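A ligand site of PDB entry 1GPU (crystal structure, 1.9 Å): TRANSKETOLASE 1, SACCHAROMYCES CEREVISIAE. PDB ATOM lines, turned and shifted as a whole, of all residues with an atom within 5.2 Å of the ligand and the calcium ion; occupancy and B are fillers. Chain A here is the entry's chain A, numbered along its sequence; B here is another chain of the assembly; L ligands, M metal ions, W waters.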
ATOM      1  N   HIS A  30      -4.800  22.238  -3.055  1.00  0.00           N
ATOM      2  CA  HIS A  30      -3.577  23.016  -3.209  1.00  0.00           C
ATOM      3  C   HIS A  30      -3.443  23.718  -4.562  1.00  0.00           C
ATOM      4  O   HIS A  30      -3.230  23.077  -5.597  1.00  0.00           O
ATOM      5  CB  HIS A  30      -2.388  22.077  -2.997  1.00  0.00           C
ATOM      6  CG  HIS A  30      -2.514  21.225  -1.777  1.00  0.00           C
ATOM      7  ND1 HIS A  30      -3.448  20.215  -1.673  1.00  0.00           N
ATOM      8  CD2 HIS A  30      -1.855  21.244  -0.591  1.00  0.00           C
ATOM      9  CE1 HIS A  30      -3.350  19.646  -0.484  1.00  0.00           C
ATOM     10  NE2 HIS A  30      -2.396  20.262   0.191  1.00  0.00           N
ATOM     11  N   ALA A  33       1.389  24.880  -6.185  1.00  0.00           N
ATOM     12  CA  ALA A  33       2.236  24.185  -7.145  1.00  0.00           C
ATOM     13  C   ALA A  33       1.615  24.095  -8.530  1.00  0.00           C
ATOM     14  O   ALA A  33       2.314  24.198  -9.534  1.00  0.00           O
ATOM     15  CB  ALA A  33       2.597  22.801  -6.621  1.00  0.00           C
ATOM     16  N   ASN A  67       4.965  15.311  -6.284  1.00  0.00           N
ATOM     17  CA  ASN A  67       4.373  16.269  -5.352  1.00  0.00           C
ATOM     18  C   ASN A  67       2.876  16.158  -5.610  1.00  0.00           C
ATOM     19  O   ASN A  67       2.238  17.044  -6.187  1.00  0.00           O
ATOM     20  CB  ASN A  67       4.899  17.696  -5.583  1.00  0.00           C
ATOM     21  CG  ASN A  67       5.029  18.081  -7.057  1.00  0.00           C
ATOM     22  OD1 ASN A  67       5.239  19.252  -7.375  1.00  0.00           O
ATOM     23  ND2 ASN A  67       4.920  17.119  -7.948  1.00  0.00           N
ATOM     24  N   HIS A  69       0.118  16.543  -3.946  1.00  0.00           N
ATOM     25  CA  HIS A  69      -0.863  17.537  -3.534  1.00  0.00           C
ATOM     26  C   HIS A  69      -1.208  18.484  -4.683  1.00  0.00           C
ATOM     27  O   HIS A  69      -2.244  19.142  -4.673  1.00  0.00           O
ATOM     28  CB  HIS A  69      -0.357  18.348  -2.327  1.00  0.00           C
ATOM     29  CG  HIS A  69       0.968  19.013  -2.556  1.00  0.00           C
ATOM     30  ND1 HIS A  69       2.170  18.341  -2.449  1.00  0.00           N
ATOM     31  CD2 HIS A  69       1.271  20.280  -2.920  1.00  0.00           C
ATOM     32  CE1 HIS A  69       3.161  19.172  -2.733  1.00  0.00           C
ATOM     33  NE2 HIS A  69       2.641  20.352  -3.026  1.00  0.00           N
ATOM     34  N   HIS A 103      -5.712  13.423  -3.829  1.00  0.00           N
ATOM     35  CA  HIS A 103      -4.347  13.074  -4.217  1.00  0.00           C
ATOM     36  C   HIS A 103      -4.498  12.028  -5.314  1.00  0.00           C
ATOM     37  O   HIS A 103      -5.477  11.283  -5.325  1.00  0.00           O
ATOM     38  CB  HIS A 103      -3.546  12.539  -3.021  1.00  0.00           C
ATOM     39  CG  HIS A 103      -3.150  13.599  -2.042  1.00  0.00           C
ATOM     40  ND1 HIS A 103      -3.953  13.974  -0.981  1.00  0.00           N
ATOM     41  CD2 HIS A 103      -2.085  14.426  -2.001  1.00  0.00           C
ATOM     42  CE1 HIS A 103      -3.408  14.993  -0.348  1.00  0.00           C
ATOM     43  NE2 HIS A 103      -2.274  15.288  -0.949  1.00  0.00           N
ATOM     44  N   GLY A 116       1.130  11.341  -2.857  1.00  0.00           N
ATOM     45  CA  GLY A 116       0.508  12.098  -1.781  1.00  0.00           C
ATOM     46  C   GLY A 116       1.531  12.001  -0.678  1.00  0.00           C
ATOM     47  O   GLY A 116       1.881  12.999  -0.046  1.00  0.00           O
ATOM     48  N   PRO A 117       2.008  10.775  -0.382  1.00  0.00           N
ATOM     49  CA  PRO A 117       3.024  10.620   0.662  1.00  0.00           C
ATOM     50  C   PRO A 117       4.310  11.030  -0.060  1.00  0.00           C
ATOM     51  O   PRO A 117       4.737  10.368  -1.011  1.00  0.00           O
ATOM     52  CB  PRO A 117       2.976   9.119   0.975  1.00  0.00           C
ATOM     53  CG  PRO A 117       1.556   8.747   0.677  1.00  0.00           C
ATOM     54  CD  PRO A 117       1.321   9.489  -0.629  1.00  0.00           C
ATOM     55  N   LEU A 118       4.900  12.141   0.377  1.00  0.00           N
ATOM     56  CA  LEU A 118       6.106  12.666  -0.261  1.00  0.00           C
ATOM     57  C   LEU A 118       7.276  11.695  -0.401  1.00  0.00           C
ATOM     58  O   LEU A 118       7.527  10.875   0.467  1.00  0.00           O
ATOM     59  CB  LEU A 118       6.563  13.931   0.480  1.00  0.00           C
ATOM     60  CG  LEU A 118       5.530  15.065   0.437  1.00  0.00           C
ATOM     61  CD1 LEU A 118       5.896  16.117   1.472  1.00  0.00           C
ATOM     62  CD2 LEU A 118       5.498  15.672  -0.953  1.00  0.00           C
ATOM     63  N   GLY A 156       8.870  18.322  -5.664  1.00  0.00           N
ATOM     64  CA  GLY A 156       9.166  19.573  -4.972  1.00  0.00           C
ATOM     65  C   GLY A 156      10.154  19.385  -3.837  1.00  0.00           C
ATOM     66  O   GLY A 156      10.779  18.335  -3.707  1.00  0.00           O
ATOM     67  N   ASP A 157      10.289  20.420  -3.009  1.00  0.00           N
ATOM     68  CA  ASP A 157      11.221  20.371  -1.878  1.00  0.00           C
ATOM     69  C   ASP A 157      10.864  19.255  -0.901  1.00  0.00           C
ATOM     70  O   ASP A 157      11.754  18.656  -0.300  1.00  0.00           O
ATOM     71  CB  ASP A 157      11.215  21.712  -1.158  1.00  0.00           C
ATOM     72  CG  ASP A 157      11.667  22.848  -2.053  1.00  0.00           C
ATOM     73  OD1 ASP A 157      12.839  22.864  -2.463  1.00  0.00           O
ATOM     74  OD2 ASP A 157      10.849  23.729  -2.351  1.00  0.00           O
ATOM     75  N   GLY A 158       9.582  18.986  -0.756  1.00  0.00           N
ATOM     76  CA  GLY A 158       9.123  17.954   0.162  1.00  0.00           C
ATOM     77  C   GLY A 158       9.671  16.588  -0.191  1.00  0.00           C
ATOM     78  O   GLY A 158      10.158  15.863   0.679  1.00  0.00           O
ATOM     79  N   CYS A 159       9.594  16.221  -1.474  1.00  0.00           N
ATOM     80  CA  CYS A 159      10.098  14.931  -1.903  1.00  0.00           C
ATOM     81  C   CYS A 159      11.605  14.852  -1.745  1.00  0.00           C
ATOM     82  O   CYS A 159      12.161  13.804  -1.386  1.00  0.00           O
ATOM     83  CB  CYS A 159       9.705  14.665  -3.367  1.00  0.00           C
ATOM     84  SG  CYS A 159       7.904  14.432  -3.617  1.00  0.00           S
ATOM     85  N   GLU A 162      12.564  13.946   1.978  1.00  0.00           N
ATOM     86  CA  GLU A 162      12.281  12.595   2.482  1.00  0.00           C
ATOM     87  C   GLU A 162      13.419  11.657   2.123  1.00  0.00           C
ATOM     88  O   GLU A 162      13.802  11.547   0.950  1.00  0.00           O
ATOM     89  CB  GLU A 162      10.977  12.068   1.880  1.00  0.00           C
ATOM     90  CG  GLU A 162       9.717  12.668   2.487  1.00  0.00           C
ATOM     91  CD  GLU A 162       9.462  12.193   3.909  1.00  0.00           C
ATOM     92  OE1 GLU A 162      10.242  11.360   4.416  1.00  0.00           O
ATOM     93  OE2 GLU A 162       8.473  12.642   4.506  1.00  0.00           O
ATOM     94  N   ASP A 185      10.530  21.497  -8.812  1.00  0.00           N
ATOM     95  CA  ASP A 185       9.847  22.778  -8.638  1.00  0.00           C
ATOM     96  C   ASP A 185      10.561  23.548  -7.526  1.00  0.00           C
ATOM     97  O   ASP A 185      10.217  23.440  -6.352  1.00  0.00           O
ATOM     98  CB  ASP A 185       8.373  22.555  -8.299  1.00  0.00           C
ATOM     99  CG  ASP A 185       7.577  23.840  -8.266  1.00  0.00           C
ATOM    100  OD1 ASP A 185       8.043  24.835  -8.863  1.00  0.00           O
ATOM    101  OD2 ASP A 185       6.478  23.868  -7.662  1.00  0.00           O
ATOM    102  N   ASN A 187      10.716  26.404  -5.766  1.00  0.00           N
ATOM    103  CA  ASN A 187       9.980  27.619  -5.402  1.00  0.00           C
ATOM    104  C   ASN A 187      10.262  28.167  -3.995  1.00  0.00           C
ATOM    105  O   ASN A 187       9.608  29.110  -3.541  1.00  0.00           O
ATOM    106  CB  ASN A 187       8.460  27.392  -5.577  1.00  0.00           C
ATOM    107  CG  ASN A 187       7.933  26.333  -4.650  1.00  0.00           C
ATOM    108  OD1 ASN A 187       8.534  26.071  -3.620  1.00  0.00           O
ATOM    109  ND2 ASN A 187       6.794  25.750  -4.993  1.00  0.00           N
ATOM    110  N   LYS A 188      11.237  27.567  -3.318  1.00  0.00           N
ATOM    111  CA  LYS A 188      11.680  27.998  -1.989  1.00  0.00           C
ATOM    112  C   LYS A 188      10.629  28.174  -0.891  1.00  0.00           C
ATOM    113  O   LYS A 188      10.788  28.996   0.020  1.00  0.00           O
ATOM    114  CB  LYS A 188      12.516  29.270  -2.147  1.00  0.00           C
ATOM    115  CG  LYS A 188      13.800  28.958  -2.915  1.00  0.00           C
ATOM    116  CD  LYS A 188      14.500  30.163  -3.455  1.00  0.00           C
ATOM    117  CE  LYS A 188      15.783  29.760  -4.166  1.00  0.00           C
ATOM    118  NZ  LYS A 188      15.556  28.835  -5.313  1.00  0.00           N
ATOM    119  N   ILE A 189       9.587  27.351  -0.947  1.00  0.00           N
ATOM    120  CA  ILE A 189       8.507  27.402   0.020  1.00  0.00           C
ATOM    121  C   ILE A 189       8.016  26.005   0.410  1.00  0.00           C
ATOM    122  O   ILE A 189       7.905  25.138  -0.439  1.00  0.00           O
ATOM    123  CB  ILE A 189       7.287  28.166  -0.542  1.00  0.00           C
ATOM    124  CG1 ILE A 189       7.565  29.677  -0.575  1.00  0.00           C
ATOM    125  CG2 ILE A 189       6.039  27.849   0.280  1.00  0.00           C
ATOM    126  CD1 ILE A 189       7.568  30.337   0.797  1.00  0.00           C
ATOM    127  N   THR A 190       7.729  25.784   1.684  1.00  0.00           N
ATOM    128  CA  THR A 190       7.151  24.533   2.128  1.00  0.00           C
ATOM    129  C   THR A 190       6.090  24.959   3.135  1.00  0.00           C
ATOM    130  O   THR A 190       5.876  26.157   3.326  1.00  0.00           O
ATOM    131  CB  THR A 190       8.175  23.560   2.789  1.00  0.00           C
ATOM    132  OG1 THR A 190       8.822  24.197   3.904  1.00  0.00           O
ATOM    133  CG2 THR A 190       9.219  23.127   1.768  1.00  0.00           C
ATOM    134  N   ILE A 191       5.406  24.010   3.762  1.00  0.00           N
ATOM    135  CA  ILE A 191       4.352  24.364   4.702  1.00  0.00           C
ATOM    136  C   ILE A 191       4.758  25.295   5.849  1.00  0.00           C
ATOM    137  O   ILE A 191       4.010  26.197   6.207  1.00  0.00           O
ATOM    138  CB  ILE A 191       3.680  23.087   5.268  1.00  0.00           C
ATOM    139  CG1 ILE A 191       2.855  22.430   4.153  1.00  0.00           C
ATOM    140  CG2 ILE A 191       2.800  23.430   6.464  1.00  0.00           C
ATOM    141  CD1 ILE A 191       2.115  21.174   4.597  1.00  0.00           C
ATOM    142  N   THR A 195      12.056  27.761   2.634  1.00  0.00           N
ATOM    143  CA  THR A 195      12.861  26.547   2.755  1.00  0.00           C
ATOM    144  C   THR A 195      14.109  26.790   3.600  1.00  0.00           C
ATOM    145  O   THR A 195      14.591  25.879   4.258  1.00  0.00           O
ATOM    146  CB  THR A 195      13.312  26.021   1.371  1.00  0.00           C
ATOM    147  OG1 THR A 195      13.852  27.095   0.594  1.00  0.00           O
ATOM    148  CG2 THR A 195      12.140  25.387   0.637  1.00  0.00           C
ATOM    149  N   ILE A 250       5.688  29.996  -6.352  1.00  0.00           N
ATOM    150  CA  ILE A 250       4.510  29.225  -5.950  1.00  0.00           C
ATOM    151  C   ILE A 250       3.281  30.131  -6.064  1.00  0.00           C
ATOM    152  O   ILE A 250       3.307  31.291  -5.664  1.00  0.00           O
ATOM    153  CB  ILE A 250       4.652  28.684  -4.499  1.00  0.00           C
ATOM    154  CG1 ILE A 250       3.533  27.686  -4.208  1.00  0.00           C
ATOM    155  CG2 ILE A 250       4.607  29.838  -3.494  1.00  0.00           C
ATOM    156  CD1 ILE A 250       3.653  27.003  -2.857  1.00  0.00           C
ATOM    157  N   HIS A 263       0.103  27.490  -0.552  1.00  0.00           N
ATOM    158  CA  HIS A 263       0.475  26.091  -0.689  1.00  0.00           C
ATOM    159  C   HIS A 263      -0.721  25.143  -0.682  1.00  0.00           C
ATOM    160  O   HIS A 263      -0.881  24.336  -1.592  1.00  0.00           O
ATOM    161  CB  HIS A 263       1.424  25.640   0.423  1.00  0.00           C
ATOM    162  CG  HIS A 263       1.381  24.166   0.686  1.00  0.00           C
ATOM    163  ND1 HIS A 263       2.075  23.256  -0.084  1.00  0.00           N
ATOM    164  CD2 HIS A 263       0.640  23.446   1.556  1.00  0.00           C
ATOM    165  CE1 HIS A 263       1.769  22.029   0.309  1.00  0.00           C
ATOM    166  NE2 HIS A 263       0.900  22.114   1.304  1.00  0.00           N
ATOM    167  N   ALA B 381       7.488  18.267  11.602  1.00  0.00           N
ATOM    168  CA  ALA B 381       8.106  17.884  10.340  1.00  0.00           C
ATOM    169  C   ALA B 381       7.384  18.657   9.234  1.00  0.00           C
ATOM    170  O   ALA B 381       6.607  18.090   8.477  1.00  0.00           O
ATOM    171  CB  ALA B 381       7.972  16.386  10.119  1.00  0.00           C
ATOM    172  N   ASP B 382       7.642  19.970   9.181  1.00  0.00           N
ATOM    173  CA  ASP B 382       7.042  20.862   8.190  1.00  0.00           C
ATOM    174  C   ASP B 382       5.513  20.932   8.253  1.00  0.00           C
ATOM    175  O   ASP B 382       4.859  21.112   7.218  1.00  0.00           O
ATOM    176  CB  ASP B 382       7.489  20.480   6.778  1.00  0.00           C
ATOM    177  CG  ASP B 382       7.267  21.607   5.772  1.00  0.00           C
ATOM    178  OD1 ASP B 382       7.715  22.740   6.029  1.00  0.00           O
ATOM    179  OD2 ASP B 382       6.644  21.350   4.719  1.00  0.00           O
ATOM    180  N   LEU B 383       4.946  20.777   9.443  1.00  0.00           N
ATOM    181  CA  LEU B 383       3.491  20.828   9.612  1.00  0.00           C
ATOM    182  C   LEU B 383       3.099  21.645  10.837  1.00  0.00           C
ATOM    183  O   LEU B 383       2.096  21.361  11.494  1.00  0.00           O
ATOM    184  CB  LEU B 383       2.909  19.416   9.724  1.00  0.00           C
ATOM    185  CG  LEU B 383       2.876  18.568   8.435  1.00  0.00           C
ATOM    186  CD1 LEU B 383       2.363  17.169   8.755  1.00  0.00           C
ATOM    187  CD2 LEU B 383       1.985  19.252   7.391  1.00  0.00           C
ATOM    188  N   ILE B 416      10.530  18.101   6.074  1.00  0.00           N
ATOM    189  CA  ILE B 416       9.783  16.873   5.775  1.00  0.00           C
ATOM    190  C   ILE B 416      10.711  15.679   5.995  1.00  0.00           C
ATOM    191  O   ILE B 416      11.150  15.011   5.047  1.00  0.00           O
ATOM    192  CB  ILE B 416       9.267  16.884   4.311  1.00  0.00           C
ATOM    193  CG1 ILE B 416       8.456  18.155   4.039  1.00  0.00           C
ATOM    194  CG2 ILE B 416       8.359  15.680   4.085  1.00  0.00           C
ATOM    195  CD1 ILE B 416       9.282  19.415   3.838  1.00  0.00           C
ATOM    196  N   GLU B 418      10.343  12.850   8.799  1.00  0.00           N
ATOM    197  CA  GLU B 418       9.785  12.151   9.957  1.00  0.00           C
ATOM    198  C   GLU B 418      10.746  11.167  10.612  1.00  0.00           C
ATOM    199  O   GLU B 418      10.920  11.170  11.826  1.00  0.00           O
ATOM    200  CB  GLU B 418       8.509  11.391   9.579  1.00  0.00           C
ATOM    201  CG  GLU B 418       7.362  12.247   9.080  1.00  0.00           C
ATOM    202  CD  GLU B 418       7.457  12.552   7.602  1.00  0.00           C
ATOM    203  OE1 GLU B 418       8.297  11.937   6.917  1.00  0.00           O
ATOM    204  OE2 GLU B 418       6.680  13.404   7.118  1.00  0.00           O
ATOM    205  N   THR B 441       3.539  15.661  13.416  1.00  0.00           N
ATOM    206  CA  THR B 441       3.339  15.245  12.031  1.00  0.00           C
ATOM    207  C   THR B 441       1.979  14.590  11.981  1.00  0.00           C
ATOM    208  O   THR B 441       1.335  14.424  13.017  1.00  0.00           O
ATOM    209  CB  THR B 441       4.405  14.236  11.537  1.00  0.00           C
ATOM    210  OG1 THR B 441       4.228  14.016  10.134  1.00  0.00           O
ATOM    211  CG2 THR B 441       4.272  12.898  12.254  1.00  0.00           C
ATOM    212  N   PHE B 442       1.517  14.230  10.790  1.00  0.00           N
ATOM    213  CA  PHE B 442       0.235  13.566  10.663  1.00  0.00           C
ATOM    214  C   PHE B 442       0.422  12.125  11.134  1.00  0.00           C
ATOM    215  O   PHE B 442       1.444  11.507  10.833  1.00  0.00           O
ATOM    216  CB  PHE B 442      -0.269  13.562   9.214  1.00  0.00           C
ATOM    217  CG  PHE B 442      -0.577  14.938   8.665  1.00  0.00           C
ATOM    218  CD1 PHE B 442      -1.100  15.933   9.491  1.00  0.00           C
ATOM    219  CD2 PHE B 442      -0.380  15.216   7.321  1.00  0.00           C
ATOM    220  CE1 PHE B 442      -1.424  17.191   8.972  1.00  0.00           C
ATOM    221  CE2 PHE B 442      -0.697  16.477   6.786  1.00  0.00           C
ATOM    222  CZ  PHE B 442      -1.225  17.464   7.615  1.00  0.00           C
ATOM    223  N   PHE B 445       1.859   9.534   8.836  1.00  0.00           N
ATOM    224  CA  PHE B 445       3.255   9.580   8.433  1.00  0.00           C
ATOM    225  C   PHE B 445       4.244   9.295   9.550  1.00  0.00           C
ATOM    226  O   PHE B 445       5.458   9.293   9.353  1.00  0.00           O
ATOM    227  CB  PHE B 445       3.527  10.908   7.705  1.00  0.00           C
ATOM    228  CG  PHE B 445       2.682  11.081   6.460  1.00  0.00           C
ATOM    229  CD1 PHE B 445       2.585  10.044   5.534  1.00  0.00           C
ATOM    230  CD2 PHE B 445       1.953  12.239   6.236  1.00  0.00           C
ATOM    231  CE1 PHE B 445       1.764  10.158   4.403  1.00  0.00           C
ATOM    232  CE2 PHE B 445       1.132  12.367   5.106  1.00  0.00           C
ATOM    233  CZ  PHE B 445       1.034  11.322   4.191  1.00  0.00           C
ATOM    234  N   TYR B 448       6.377   6.540   8.671  1.00  0.00           N
ATOM    235  CA  TYR B 448       7.608   6.751   7.904  1.00  0.00           C
ATOM    236  C   TYR B 448       8.804   6.633   8.840  1.00  0.00           C
ATOM    237  O   TYR B 448       9.941   6.415   8.395  1.00  0.00           O
ATOM    238  CB  TYR B 448       7.635   8.151   7.286  1.00  0.00           C
ATOM    239  CG  TYR B 448       7.258   8.243   5.816  1.00  0.00           C
ATOM    240  CD1 TYR B 448       6.035   7.767   5.343  1.00  0.00           C
ATOM    241  CD2 TYR B 448       8.123   8.862   4.905  1.00  0.00           C
ATOM    242  CE1 TYR B 448       5.680   7.920   3.994  1.00  0.00           C
ATOM    243  CE2 TYR B 448       7.773   9.015   3.565  1.00  0.00           C
ATOM    244  CZ  TYR B 448       6.548   8.550   3.118  1.00  0.00           C
ATOM    245  OH  TYR B 448       6.189   8.757   1.798  1.00  0.00           O
ATOM    246  N   ASP B 477      -8.206  15.143   1.870  1.00  0.00           N
ATOM    247  CA  ASP B 477      -6.895  14.656   1.463  1.00  0.00           C
ATOM    248  C   ASP B 477      -6.946  13.197   1.042  1.00  0.00           C
ATOM    249  O   ASP B 477      -6.091  12.733   0.282  1.00  0.00           O
ATOM    250  CB  ASP B 477      -5.860  14.887   2.574  1.00  0.00           C
ATOM    251  CG  ASP B 477      -5.321  16.308   2.565  1.00  0.00           C
ATOM    252  OD1 ASP B 477      -5.531  17.002   1.554  1.00  0.00           O
ATOM    253  OD2 ASP B 477      -4.697  16.728   3.551  1.00  0.00           O
ATOM    254  N   HIS B 481      -3.744   9.771   3.218  1.00  0.00           N
ATOM    255  CA  HIS B 481      -3.533  10.567   4.431  1.00  0.00           C
ATOM    256  C   HIS B 481      -4.350  10.096   5.618  1.00  0.00           C
ATOM    257  O   HIS B 481      -4.210  10.627   6.722  1.00  0.00           O
ATOM    258  CB  HIS B 481      -3.871  12.035   4.173  1.00  0.00           C
ATOM    259  CG  HIS B 481      -2.822  12.775   3.397  1.00  0.00           C
ATOM    260  ND1 HIS B 481      -2.358  12.342   2.165  1.00  0.00           N
ATOM    261  CD2 HIS B 481      -2.149  13.915   3.671  1.00  0.00           C
ATOM    262  CE1 HIS B 481      -1.451  13.190   1.721  1.00  0.00           C
ATOM    263  NE2 HIS B 481      -1.307  14.155   2.613  1.00  0.00           N
HETATM  264  N1  LIG L   1       4.989  13.571   5.153  1.00  0.00           N
HETATM  265  C1  LIG L   1       4.802  12.808   4.058  1.00  0.00           C
HETATM  266  C2  LIG L   1       5.578  11.594   3.921  1.00  0.00           C
HETATM  267  N2  LIG L   1       3.930  13.169   3.131  1.00  0.00           N
HETATM  268  C3  LIG L   1       3.175  14.341   3.264  1.00  0.00           C
HETATM  269  N3  LIG L   1       2.331  14.576   2.264  1.00  0.00           N
HETATM  270  C4  LIG L   1       3.330  15.209   4.434  1.00  0.00           C
HETATM  271  C5  LIG L   1       4.273  14.749   5.332  1.00  0.00           C
HETATM  272  C6  LIG L   1       2.562  16.518   4.691  1.00  0.00           C
HETATM  273  N4  LIG L   1       2.778  17.482   3.488  1.00  0.00           N
HETATM  274  C7  LIG L   1       1.953  17.666   2.364  1.00  0.00           C
HETATM  275  S1  LIG L   1       2.655  18.775   1.260  1.00  0.00           S
HETATM  276  C8  LIG L   1       3.985  19.022   2.279  1.00  0.00           C
HETATM  277  C9  LIG L   1       3.884  18.259   3.414  1.00  0.00           C
HETATM  278  C10 LIG L   1       4.907  18.257   4.497  1.00  0.00           C
HETATM  279  C11 LIG L   1       5.109  19.977   1.923  1.00  0.00           C
HETATM  280  C12 LIG L   1       4.868  20.841   0.747  1.00  0.00           C
HETATM  281  O1  LIG L   1       6.164  21.193   0.270  1.00  0.00           O
HETATM  282  P1  LIG L   1       6.489  20.844  -1.202  1.00  0.00           P
HETATM  283  O2  LIG L   1       6.638  19.385  -1.542  1.00  0.00           O
HETATM  284  O3  LIG L   1       7.650  21.671  -1.312  1.00  0.00           O
HETATM  285  O4  LIG L   1       5.531  21.709  -2.169  1.00  0.00           O
HETATM  286  P2  LIG L   1       4.807  23.131  -2.396  1.00  0.00           P
HETATM  287  O5  LIG L   1       5.895  23.729  -3.144  1.00  0.00           O
HETATM  288  O6  LIG L   1       3.660  22.853  -3.250  1.00  0.00           O
HETATM  289  O7  LIG L   1       4.412  23.704  -1.084  1.00  0.00           O
HETATM  290  C13 LIG L   1       0.816  17.103   2.409  1.00  0.00           C
HETATM  291  O8  LIG L   1       0.247  16.409   3.284  1.00  0.00           O
HETATM  292  C14 LIG L   1       0.136  17.394   1.166  1.00  0.00           C
HETATM  293  O9  LIG L   1      -0.036  16.200   0.416  1.00  0.00           O
HETATM  294 CA    CA M   1       8.338  23.897  -2.402  1.00  0.00          CA
HETATM  295  O   HOH W   1       2.099  15.736  -1.627  1.00  0.00           O
HETATM  296  O   HOH W   2       5.996  21.852  -5.855  1.00  0.00           O
HETATM  297  O   HOH W   3       8.620  22.444  -4.720  1.00  0.00           O
HETATM  298  O   HOH W   4       5.482  15.622   8.206  1.00  0.00           O
HETATM  299  O   HOH W   5       7.628  17.472  -3.286  1.00  0.00           O
HETATM  300  O   HOH W   6       1.012  23.670  -3.565  1.00  0.00           O
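O of Asp 477 of chain B lies within hydrogen-bond range of ND1 of His 103 (2.8 Å).
The backbone carbonyl oxygen of Leu 118 lies within hydrogen-bond range of the side-chain hydroxyl of Tyr 448 of chain B, 2.8 Å away.
OD1 of Asp 382 of chain B lies within hydrogen-bond range of OG1 of Thr 190 (2.8 Å).
OD2 of Asp 382 of chain B is in hydrogen-bond range of N of Ile 191, 3.1 Å away.
The backbone carbonyl oxygen (O) of His 69 sits close to a ring nitrogen (ND1) of His 30 (3.4 Å).
The side-chain carboxylate (OE2) of Glu 162 sits close to the side-chain carboxylate (OE1) of Glu 418 of chain B (2.5 Å).
OD2 of Asp 185 lies within hydrogen-bond range of ND2 of Asn 187 (3.3 Å).
Residues that only touch the ligand: His 30, Ala 33, Pro 117, Glu 162, Thr 190, Ile 191, Ile 250, Asp 382 of chain B, Leu 383 of chain B, Ile 416 of chain B, Phe 442 of chain B, Phe 445 of chain B and Tyr 448 of chain B.
Within 4 Å of the ligand: His 30, Ala 33, His 69, His 103, Gly 116, Pro 117, Leu 118, Asp 157, Gly 158, Glu 162, Asn 187, Ile 189, Thr 190, Ile 191, Ile 250, His 263, Asp 382 of chain B, Leu 383 of chain B, Ile 416 of chain B, Glu 418 of chain B, Phe 442 of chain B, Phe 445 of chain B, Tyr 448 of chain B and His 481 of chain B.
The nearest printed residue that does not touch the ligand is Gly 156 (4.2 Å).
Three residues have an atom within 4 Å of the calcium ion: Asp 157, Asn 187 and Ile 189.
The nearest printed residue that does not touch the calcium ion is Thr 190 (4.3 Å).
A ring nitrogen (NE2) of His 481 of chain B lies within hydrogen-bond range of an oxygen (O8) of the ligand (2.8 Å).
The backbone NH (N) of Asp 157 sits close to an oxygen (O3) of the ligand, at 3.4 Å.
N of Leu 118 lies within hydrogen-bond range of N2 of the ligand, at 3.1 Å.
NE2 of His 69 sits at hydrogen-bond distance from O6 of the ligand (2.7 Å).
O7 of the ligand sits at hydrogen-bond distance from ND1 of His 263.
A ring nitrogen (NE2) of His 103 is in hydrogen-bond range of an oxygen (O9) of the ligand.
OE2 of Glu 418 of chain B lies within hydrogen-bond range of N1 of the ligand, 2.6 Å away.
The backbone NH of Gly 158 lies within hydrogen-bond range of an oxygen (O2) of the ligand (3.1 Å).
O of Gly 116 sits at hydrogen-bond distance from N3 of the ligand.
Water W3 lies within hydrogen-bond range of O of Asp 185 and N of Asp 157.
Water W5 lies within hydrogen-bond range of O2 of the ligand (2.8 Å), N of Gly 156 (2.8 Å) and N of Cys 159 (3.0 Å).
Water W6 lies within hydrogen-bond range of an oxygen (O6) of the ligand, the backbone carbonyl oxygen of His 263 and the backbone NH of Ala 33.
Water W1 lies within hydrogen-bond range of a ring nitrogen (ND1) of His 69 (2.7 Å), an oxygen (O9) of the ligand (3.0 Å) and the backbone carbonyl oxygen (O) of Gly 116 (3.2 Å).
Water W4 lies within hydrogen-bond range of O of Ala 381 of chain B, OE2 of Glu 418 of chain B and OG1 of Thr 441 of chain B.
Water W2 bridges OD2 of Asp 185 (2.7 Å) and OD1 of Asn 67 (3.1 Å).
The calcium ion is bound by O of Ile 189 (2.4 Å).
OD1 of Asn 187 is bound to the calcium ion (2.5 Å).
The calcium ion is bound by OD2 of Asp 157 (2.5 Å).
An oxygen (O5) of the ligand is bound to the calcium ion (2.6 Å).
The calcium ion is bound by O3 of the ligand.
The calcium ion is bound by water W3 (2.8 Å).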
